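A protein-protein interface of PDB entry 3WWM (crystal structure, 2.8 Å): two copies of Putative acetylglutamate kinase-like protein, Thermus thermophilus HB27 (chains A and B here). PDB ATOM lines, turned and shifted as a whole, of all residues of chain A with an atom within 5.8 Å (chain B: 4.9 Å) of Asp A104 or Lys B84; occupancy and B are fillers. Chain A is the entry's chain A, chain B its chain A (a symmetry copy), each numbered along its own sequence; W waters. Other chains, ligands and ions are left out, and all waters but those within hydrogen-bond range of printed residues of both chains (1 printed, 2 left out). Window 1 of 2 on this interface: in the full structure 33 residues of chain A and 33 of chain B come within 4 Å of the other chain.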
ATOM      1  N   GLU A  75     -18.360  -3.689  33.336  1.00  0.00           N
ATOM      2  CA  GLU A  75     -17.986  -2.671  32.360  1.00  0.00           C
ATOM      3  C   GLU A  75     -18.042  -1.268  32.950  1.00  0.00           C
ATOM      4  O   GLU A  75     -17.125  -0.477  32.747  1.00  0.00           O
ATOM      5  CB  GLU A  75     -18.848  -2.774  31.101  1.00  0.00           C
ATOM      6  CG  GLU A  75     -18.466  -3.971  30.248  1.00  0.00           C
ATOM      7  CD  GLU A  75     -19.349  -4.165  29.042  1.00  0.00           C
ATOM      8  OE1 GLU A  75     -20.522  -3.734  29.075  1.00  0.00           O
ATOM      9  OE2 GLU A  75     -18.863  -4.765  28.059  1.00  0.00           O
ATOM     10  N   CYS A  79     -14.084  -0.543  33.081  1.00  0.00           N
ATOM     11  CA  CYS A  79     -13.905   0.258  31.879  1.00  0.00           C
ATOM     12  C   CYS A  79     -14.252   1.726  32.088  1.00  0.00           C
ATOM     13  O   CYS A  79     -13.740   2.588  31.376  1.00  0.00           O
ATOM     14  CB  CYS A  79     -14.747  -0.309  30.737  1.00  0.00           C
ATOM     15  SG  CYS A  79     -14.445  -2.059  30.392  1.00  0.00           S
ATOM     16  N   LYS A  84     -10.702   5.185  33.682  1.00  0.00           N
ATOM     17  CA  LYS A  84     -10.633   6.639  33.525  1.00  0.00           C
ATOM     18  C   LYS A  84     -10.032   7.355  34.738  1.00  0.00           C
ATOM     19  O   LYS A  84      -9.395   8.399  34.585  1.00  0.00           O
ATOM     20  CB  LYS A  84     -12.008   7.216  33.185  1.00  0.00           C
ATOM     21  CG  LYS A  84     -12.692   6.567  31.979  1.00  0.00           C
ATOM     22  CD  LYS A  84     -11.752   6.312  30.814  1.00  0.00           C
ATOM     23  CE  LYS A  84     -12.489   5.695  29.644  1.00  0.00           C
ATOM     24  NZ  LYS A  84     -11.551   5.288  28.561  1.00  0.00           N
ATOM     25  N   GLY A  99      -6.617   4.789  27.631  1.00  0.00           N
ATOM     26  CA  GLY A  99      -7.338   3.689  28.243  1.00  0.00           C
ATOM     27  C   GLY A  99      -8.107   2.911  27.199  1.00  0.00           C
ATOM     28  O   GLY A  99      -8.793   3.500  26.361  1.00  0.00           O
ATOM     29  N   LEU A 100      -7.989   1.588  27.254  1.00  0.00           N
ATOM     30  CA  LEU A 100      -8.640   0.702  26.299  1.00  0.00           C
ATOM     31  C   LEU A 100      -9.097  -0.573  26.991  1.00  0.00           C
ATOM     32  O   LEU A 100      -8.434  -1.045  27.909  1.00  0.00           O
ATOM     33  CB  LEU A 100      -7.663   0.335  25.181  1.00  0.00           C
ATOM     34  CG  LEU A 100      -7.263   1.442  24.206  1.00  0.00           C
ATOM     35  CD1 LEU A 100      -6.222   0.920  23.231  1.00  0.00           C
ATOM     36  CD2 LEU A 100      -8.475   1.968  23.455  1.00  0.00           C
ATOM     37  N   SER A 101     -10.230  -1.117  26.555  1.00  0.00           N
ATOM     38  CA  SER A 101     -10.677  -2.434  26.997  1.00  0.00           C
ATOM     39  C   SER A 101     -10.348  -3.451  25.916  1.00  0.00           C
ATOM     40  O   SER A 101      -9.980  -3.080  24.797  1.00  0.00           O
ATOM     41  CB  SER A 101     -12.180  -2.440  27.254  1.00  0.00           C
ATOM     42  OG  SER A 101     -12.921  -2.576  26.040  1.00  0.00           O
ATOM     43  N   GLY A 102     -10.518  -4.731  26.225  1.00  0.00           N
ATOM     44  CA  GLY A 102     -10.279  -5.787  25.237  1.00  0.00           C
ATOM     45  C   GLY A 102     -11.208  -5.744  24.042  1.00  0.00           C
ATOM     46  O   GLY A 102     -10.917  -6.322  23.005  1.00  0.00           O
ATOM     47  N   LEU A 103     -12.336  -5.060  24.192  1.00  0.00           N
ATOM     48  CA  LEU A 103     -13.307  -4.915  23.119  1.00  0.00           C
ATOM     49  C   LEU A 103     -12.826  -3.931  22.064  1.00  0.00           C
ATOM     50  O   LEU A 103     -13.180  -4.042  20.884  1.00  0.00           O
ATOM     51  CB  LEU A 103     -14.617  -4.393  23.685  1.00  0.00           C
ATOM     52  CG  LEU A 103     -15.255  -5.204  24.804  1.00  0.00           C
ATOM     53  CD1 LEU A 103     -16.297  -4.359  25.507  1.00  0.00           C
ATOM     54  CD2 LEU A 103     -15.880  -6.466  24.244  1.00  0.00           C
ATOM     55  N   ASP A 104     -12.024  -2.965  22.496  1.00  0.00           N
ATOM     56  CA  ASP A 104     -11.656  -1.840  21.649  1.00  0.00           C
ATOM     57  C   ASP A 104     -10.580  -2.219  20.640  1.00  0.00           C
ATOM     58  O   ASP A 104      -9.471  -2.592  21.010  1.00  0.00           O
ATOM     59  CB  ASP A 104     -11.207  -0.677  22.521  1.00  0.00           C
ATOM     60  CG  ASP A 104     -12.330  -0.158  23.390  1.00  0.00           C
ATOM     61  OD1 ASP A 104     -13.308   0.378  22.821  1.00  0.00           O
ATOM     62  OD2 ASP A 104     -12.248  -0.300  24.627  1.00  0.00           O
ATOM     63  N   GLY A 105     -10.920  -2.138  19.360  1.00  0.00           N
ATOM     64  CA  GLY A 105     -10.001  -2.542  18.311  1.00  0.00           C
ATOM     65  C   GLY A 105      -9.758  -4.042  18.294  1.00  0.00           C
ATOM     66  O   GLY A 105      -8.782  -4.498  17.705  1.00  0.00           O
ATOM     67  N   ARG A 106     -10.656  -4.807  18.925  1.00  0.00           N
ATOM     68  CA  ARG A 106     -10.477  -6.249  19.133  1.00  0.00           C
ATOM     69  C   ARG A 106      -9.140  -6.541  19.818  1.00  0.00           C
ATOM     70  O   ARG A 106      -8.448  -7.493  19.485  1.00  0.00           O
ATOM     71  CB  ARG A 106     -10.618  -7.018  17.815  1.00  0.00           C
ATOM     72  CG  ARG A 106     -11.953  -6.791  17.120  1.00  0.00           C
ATOM     73  CD  ARG A 106     -12.009  -7.380  15.714  1.00  0.00           C
ATOM     74  NE  ARG A 106     -11.588  -8.779  15.685  1.00  0.00           N
ATOM     75  CZ  ARG A 106     -12.309  -9.803  16.144  1.00  0.00           C
ATOM     76  NH1 ARG A 106     -13.508  -9.607  16.680  1.00  0.00           N
ATOM     77  NH2 ARG A 106     -11.828 -11.041  16.070  1.00  0.00           N
ATOM     78  N   LEU A 107      -8.802  -5.713  20.797  1.00  0.00           N
ATOM     79  CA  LEU A 107      -7.517  -5.797  21.477  1.00  0.00           C
ATOM     80  C   LEU A 107      -7.256  -7.161  22.124  1.00  0.00           C
ATOM     81  O   LEU A 107      -6.170  -7.717  21.967  1.00  0.00           O
ATOM     82  CB  LEU A 107      -7.397  -4.685  22.522  1.00  0.00           C
ATOM     83  CG  LEU A 107      -6.104  -4.682  23.332  1.00  0.00           C
ATOM     84  CD1 LEU A 107      -4.886  -4.501  22.438  1.00  0.00           C
ATOM     85  CD2 LEU A 107      -6.166  -3.586  24.382  1.00  0.00           C
ATOM     86  N   PHE A 108      -8.240  -7.682  22.858  1.00  0.00           N
ATOM     87  CA  PHE A 108      -8.135  -8.993  23.490  1.00  0.00           C
ATOM     88  C   PHE A 108      -9.271  -9.874  23.000  1.00  0.00           C
ATOM     89  O   PHE A 108     -10.443  -9.518  23.148  1.00  0.00           O
ATOM     90  CB  PHE A 108      -8.204  -8.890  25.013  1.00  0.00           C
ATOM     91  CG  PHE A 108      -7.183  -7.968  25.614  1.00  0.00           C
ATOM     92  CD1 PHE A 108      -5.849  -8.044  25.241  1.00  0.00           C
ATOM     93  CD2 PHE A 108      -7.552  -7.038  26.575  1.00  0.00           C
ATOM     94  CE1 PHE A 108      -4.910  -7.197  25.799  1.00  0.00           C
ATOM     95  CE2 PHE A 108      -6.619  -6.188  27.136  1.00  0.00           C
ATOM     96  CZ  PHE A 108      -5.294  -6.265  26.743  1.00  0.00           C
ATOM     97  N   ASN A 139      -4.302  -7.772  19.869  1.00  0.00           N
ATOM     98  CA  ASN A 139      -4.081  -6.921  18.707  1.00  0.00           C
ATOM     99  C   ASN A 139      -2.803  -6.142  18.956  1.00  0.00           C
ATOM    100  O   ASN A 139      -2.828  -4.961  19.303  1.00  0.00           O
ATOM    101  CB  ASN A 139      -5.272  -5.996  18.452  1.00  0.00           C
ATOM    102  CG  ASN A 139      -5.098  -5.150  17.208  1.00  0.00           C
ATOM    103  OD1 ASN A 139      -4.055  -5.172  16.562  1.00  0.00           O
ATOM    104  ND2 ASN A 139      -6.122  -4.381  16.878  1.00  0.00           N
ATOM    105  N   LEU A 142      -2.087  -2.766  17.110  1.00  0.00           N
ATOM    106  CA  LEU A 142      -2.679  -1.575  17.708  1.00  0.00           C
ATOM    107  C   LEU A 142      -1.827  -1.064  18.857  1.00  0.00           C
ATOM    108  O   LEU A 142      -1.515   0.122  18.923  1.00  0.00           O
ATOM    109  CB  LEU A 142      -4.092  -1.877  18.194  1.00  0.00           C
ATOM    110  CG  LEU A 142      -4.792  -0.755  18.956  1.00  0.00           C
ATOM    111  CD1 LEU A 142      -4.950   0.481  18.084  1.00  0.00           C
ATOM    112  CD2 LEU A 142      -6.140  -1.253  19.460  1.00  0.00           C
ATOM    113  N   CYS B  79     -18.654   6.142  29.712  1.00  0.00           N
ATOM    114  CA  CYS B  79     -17.392   5.527  29.328  1.00  0.00           C
ATOM    115  C   CYS B  79     -17.393   4.015  29.502  1.00  0.00           C
ATOM    116  O   CYS B  79     -16.642   3.315  28.824  1.00  0.00           O
ATOM    117  CB  CYS B  79     -16.243   6.134  30.133  1.00  0.00           C
ATOM    118  SG  CYS B  79     -16.135   7.936  30.027  1.00  0.00           S
ATOM    119  N   GLY B  80     -18.226   3.511  30.409  1.00  0.00           N
ATOM    120  CA  GLY B  80     -18.281   2.081  30.689  1.00  0.00           C
ATOM    121  C   GLY B  80     -19.414   1.372  29.976  1.00  0.00           C
ATOM    122  O   GLY B  80     -19.191   0.631  29.025  1.00  0.00           O
ATOM    123  N   LEU B  81     -20.636   1.606  30.438  1.00  0.00           N
ATOM    124  CA  LEU B  81     -21.809   0.904  29.917  1.00  0.00           C
ATOM    125  C   LEU B  81     -22.091   1.206  28.434  1.00  0.00           C
ATOM    126  O   LEU B  81     -22.127   0.296  27.605  1.00  0.00           O
ATOM    127  CB  LEU B  81     -23.035   1.250  30.768  1.00  0.00           C
ATOM    128  CG  LEU B  81     -24.291   0.412  30.527  1.00  0.00           C
ATOM    129  CD1 LEU B  81     -24.079  -1.028  30.957  1.00  0.00           C
ATOM    130  CD2 LEU B  81     -25.467   1.022  31.267  1.00  0.00           C
ATOM    131  N   VAL B  82     -22.274   2.479  28.105  1.00  0.00           N
ATOM    132  CA  VAL B  82     -22.702   2.856  26.763  1.00  0.00           C
ATOM    133  C   VAL B  82     -21.584   2.684  25.733  1.00  0.00           C
ATOM    134  O   VAL B  82     -21.789   2.080  24.682  1.00  0.00           O
ATOM    135  CB  VAL B  82     -23.224   4.310  26.708  1.00  0.00           C
ATOM    136  CG1 VAL B  82     -23.673   4.658  25.297  1.00  0.00           C
ATOM    137  CG2 VAL B  82     -24.383   4.509  27.672  1.00  0.00           C
ATOM    138  N   ASN B  83     -20.408   3.228  26.027  1.00  0.00           N
ATOM    139  CA  ASN B  83     -19.279   3.155  25.098  1.00  0.00           C
ATOM    140  C   ASN B  83     -18.988   1.707  24.709  1.00  0.00           C
ATOM    141  O   ASN B  83     -18.861   1.400  23.528  1.00  0.00           O
ATOM    142  CB  ASN B  83     -18.039   3.831  25.712  1.00  0.00           C
ATOM    143  CG  ASN B  83     -16.874   3.944  24.742  1.00  0.00           C
ATOM    144  OD1 ASN B  83     -15.957   3.131  24.767  1.00  0.00           O
ATOM    145  ND2 ASN B  83     -16.891   4.963  23.905  1.00  0.00           N
ATOM    146  N   LYS B  84     -18.931   0.814  25.693  1.00  0.00           N
ATOM    147  CA  LYS B  84     -18.614  -0.590  25.427  1.00  0.00           C
ATOM    148  C   LYS B  84     -19.792  -1.380  24.848  1.00  0.00           C
ATOM    149  O   LYS B  84     -19.584  -2.315  24.072  1.00  0.00           O
ATOM    150  CB  LYS B  84     -18.072  -1.274  26.682  1.00  0.00           C
ATOM    151  CG  LYS B  84     -16.885  -0.560  27.335  1.00  0.00           C
ATOM    152  CD  LYS B  84     -15.860  -0.051  26.336  1.00  0.00           C
ATOM    153  CE  LYS B  84     -14.700   0.620  27.041  1.00  0.00           C
ATOM    154  NZ  LYS B  84     -13.772   1.268  26.072  1.00  0.00           N
ATOM    155  N   ARG B  85     -21.020  -1.017  25.212  1.00  0.00           N
ATOM    156  CA  ARG B  85     -22.191  -1.582  24.539  1.00  0.00           C
ATOM    157  C   ARG B  85     -22.082  -1.310  23.046  1.00  0.00           C
ATOM    158  O   ARG B  85     -22.211  -2.214  22.216  1.00  0.00           O
ATOM    159  CB  ARG B  85     -23.482  -0.961  25.058  1.00  0.00           C
ATOM    160  CG  ARG B  85     -24.740  -1.466  24.362  1.00  0.00           C
ATOM    161  CD  ARG B  85     -25.923  -0.581  24.694  1.00  0.00           C
ATOM    162  NE  ARG B  85     -26.260  -0.628  26.116  1.00  0.00           N
ATOM    163  CZ  ARG B  85     -26.761   0.388  26.818  1.00  0.00           C
ATOM    164  NH1 ARG B  85     -26.976   1.566  26.258  1.00  0.00           N
ATOM    165  NH2 ARG B  85     -27.035   0.236  28.103  1.00  0.00           N
ATOM    166  N   LEU B  86     -21.826  -0.053  22.721  1.00  0.00           N
ATOM    167  CA  LEU B  86     -21.757   0.383  21.338  1.00  0.00           C
ATOM    168  C   LEU B  86     -20.607  -0.307  20.594  1.00  0.00           C
ATOM    169  O   LEU B  86     -20.795  -0.777  19.470  1.00  0.00           O
ATOM    170  CB  LEU B  86     -21.613   1.904  21.294  1.00  0.00           C
ATOM    171  CG  LEU B  86     -22.148   2.694  20.107  1.00  0.00           C
ATOM    172  CD1 LEU B  86     -23.321   2.027  19.399  1.00  0.00           C
ATOM    173  CD2 LEU B  86     -22.533   4.084  20.598  1.00  0.00           C
ATOM    174  N   VAL B  87     -19.437  -0.392  21.231  1.00  0.00           N
ATOM    175  CA  VAL B  87     -18.283  -1.055  20.628  1.00  0.00           C
ATOM    176  C   VAL B  87     -18.574  -2.537  20.393  1.00  0.00           C
ATOM    177  O   VAL B  87     -18.271  -3.068  19.320  1.00  0.00           O
ATOM    178  CB  VAL B  87     -17.011  -0.899  21.487  1.00  0.00           C
ATOM    179  CG1 VAL B  87     -15.914  -1.844  21.013  1.00  0.00           C
ATOM    180  CG2 VAL B  87     -16.508   0.534  21.443  1.00  0.00           C
ATOM    181  N   GLU B  88     -19.163  -3.203  21.385  1.00  0.00           N
ATOM    182  CA  GLU B  88     -19.511  -4.615  21.230  1.00  0.00           C
ATOM    183  C   GLU B  88     -20.474  -4.799  20.072  1.00  0.00           C
ATOM    184  O   GLU B  88     -20.267  -5.662  19.225  1.00  0.00           O
ATOM    185  CB  GLU B  88     -20.133  -5.188  22.504  1.00  0.00           C
ATOM    186  CG  GLU B  88     -20.607  -6.631  22.347  1.00  0.00           C
ATOM    187  CD  GLU B  88     -21.145  -7.234  23.633  1.00  0.00           C
ATOM    188  OE1 GLU B  88     -21.403  -6.494  24.603  1.00  0.00           O
ATOM    189  OE2 GLU B  88     -21.313  -8.465  23.676  1.00  0.00           O
ATOM    190  N   LEU B  89     -21.529  -3.986  20.048  1.00  0.00           N
ATOM    191  CA  LEU B  89     -22.540  -4.077  18.989  1.00  0.00           C
ATOM    192  C   LEU B  89     -21.904  -3.902  17.613  1.00  0.00           C
ATOM    193  O   LEU B  89     -22.213  -4.652  16.687  1.00  0.00           O
ATOM    194  CB  LEU B  89     -23.650  -3.042  19.196  1.00  0.00           C
ATOM    195  CG  LEU B  89     -24.639  -3.307  20.341  1.00  0.00           C
ATOM    196  CD1 LEU B  89     -25.442  -2.052  20.657  1.00  0.00           C
ATOM    197  CD2 LEU B  89     -25.565  -4.457  20.007  1.00  0.00           C
ATOM    198  N   ALA B  97     -14.655  -1.243  15.804  1.00  0.00           N
ATOM    199  CA  ALA B  97     -14.827  -0.012  16.554  1.00  0.00           C
ATOM    200  C   ALA B  97     -13.791   0.101  17.654  1.00  0.00           C
ATOM    201  O   ALA B  97     -13.321  -0.903  18.189  1.00  0.00           O
ATOM    202  CB  ALA B  97     -16.222   0.073  17.153  1.00  0.00           C
ATOM    203  N   ILE B  98     -13.448   1.340  17.983  1.00  0.00           N
ATOM    204  CA  ILE B  98     -12.547   1.624  19.079  1.00  0.00           C
ATOM    205  C   ILE B  98     -13.181   2.742  19.904  1.00  0.00           C
ATOM    206  O   ILE B  98     -13.500   3.813  19.388  1.00  0.00           O
ATOM    207  CB  ILE B  98     -11.134   1.966  18.566  1.00  0.00           C
ATOM    208  CG1 ILE B  98     -10.118   1.931  19.690  1.00  0.00           C
ATOM    209  CG2 ILE B  98     -11.084   3.328  17.894  1.00  0.00           C
ATOM    210  CD1 ILE B  98      -8.706   2.031  19.165  1.00  0.00           C
ATOM    211  N   GLY B  99     -13.416   2.449  21.180  1.00  0.00           N
ATOM    212  CA  GLY B  99     -14.075   3.371  22.085  1.00  0.00           C
ATOM    213  C   GLY B  99     -13.055   4.181  22.853  1.00  0.00           C
ATOM    214  O   GLY B  99     -12.088   3.628  23.382  1.00  0.00           O
HETATM  215  O   HOH W   1     -22.551  -2.429  28.166  1.00  0.00           O
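Water W1 lies within hydrogen-bond range of the side-chain carboxylate of Glu A75 (2.6 Å) and the backbone carbonyl oxygen of Leu B81 (2.8 Å).
The side-chain carboxylate (OD1) of Asp A104 sits at hydrogen-bond distance from the backbone NH (N) of Gly B99. The backbone carbonyl oxygen (O) of Ala B97 lies within hydrogen-bond range of the backbone NH (N) of Gly A105 (2.9 Å). The side-chain amino group (NZ) of Lys B84 is in salt-bridge range of the side-chain carboxylate (OD2) of Asp A104.
Cys A79 touches its own counterpart, Cys B79. Cys A79 touches Lys B84, and with the chains exchanged Lys A84 touches Cys B79. Of the 15 pairs that touch across the chains among the printed residues, 3 have their exchanged pair printed and touching as well.
Of the 14 printed residues of chain B, 7 touch a printed residue of chain A. Hydrophobic or aromatic side chains of chain B within 4 Å of the printed part of chain A: Val B87. Hydrophobic or aromatic side chains of chain A within 4 Å of the printed part of chain B: Leu A100 and Leu A103. Among the printed residues, 15 pairs touch across the chains. Among the printed residues, Asp or Glu carboxylates within 4 Å of a Lys or Arg side-chain nitrogen of the other chain: Asp A104 with Lys B84 (2.6 Å).
Among the printed residues, pairs that only touch across the chains: Glu A75 with Gly B80 (3.5 Å), Asp A104 with Val B87 (3.5 Å), Leu A103 with Val B87 (3.5 Å), Leu A103 with Lys B84 (3.7 Å), Asp A104 with Ile B98 (3.8 Å), Ser A101 with Lys B84 (3.8 Å), Lys A84 with Cys B79 (3.8 Å), Cys A79 with Lys B84 (3.8 Å), Glu A75 with Lys B84 (3.8 Å), Asp A104 with Ala B97 (3.9 Å), Cys A79 with Cys B79 (3.9 Å) and Leu A100 with Gly B99 (3.98 Å).
The backbone carbonyl oxygen (O) of Gly A105 lies within hydrogen-bond range of the side-chain amide nitrogen (ND2) of Asn A139 (2.8 Å). The side-chain carboxylate of Asp A104 lies within hydrogen-bond range of the side-chain hydroxyl of Ser A101, at 2.8 Å. The side-chain hydroxyl of Ser A101 sits close to the backbone NH of Leu A103. The side-chain amide oxygen (OD1) of Asn B83 is in hydrogen-bond range of the side-chain amino group (NZ) of Lys B84 (3.2 Å).
Of the printed residues of chain B, Ser A101 touches Lys B84. Of the printed residues of chain A, Cys B79 touches Cys A79 and Lys A84. Lys B84 touches just these residues of chain A: Glu A75 (3.8 Å), Cys A79 (3.8 Å), Ser A101 (3.8 Å), Leu A103 (3.7 Å) and Asp A104 (2.6 Å). Arg B85 touches none of the printed residues of chain A. Glu B88 touches none of the printed residues of chain A. Of the printed residues of chain A, Ile B98 touches Asp A104 (3.8 Å). The nearest residue of chain A that does not touch Lys B84 is Leu A100 (5.1 Å). The nearest printed residue of chain A that does not touch Ala B97 is Leu A103 (4.1 Å).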
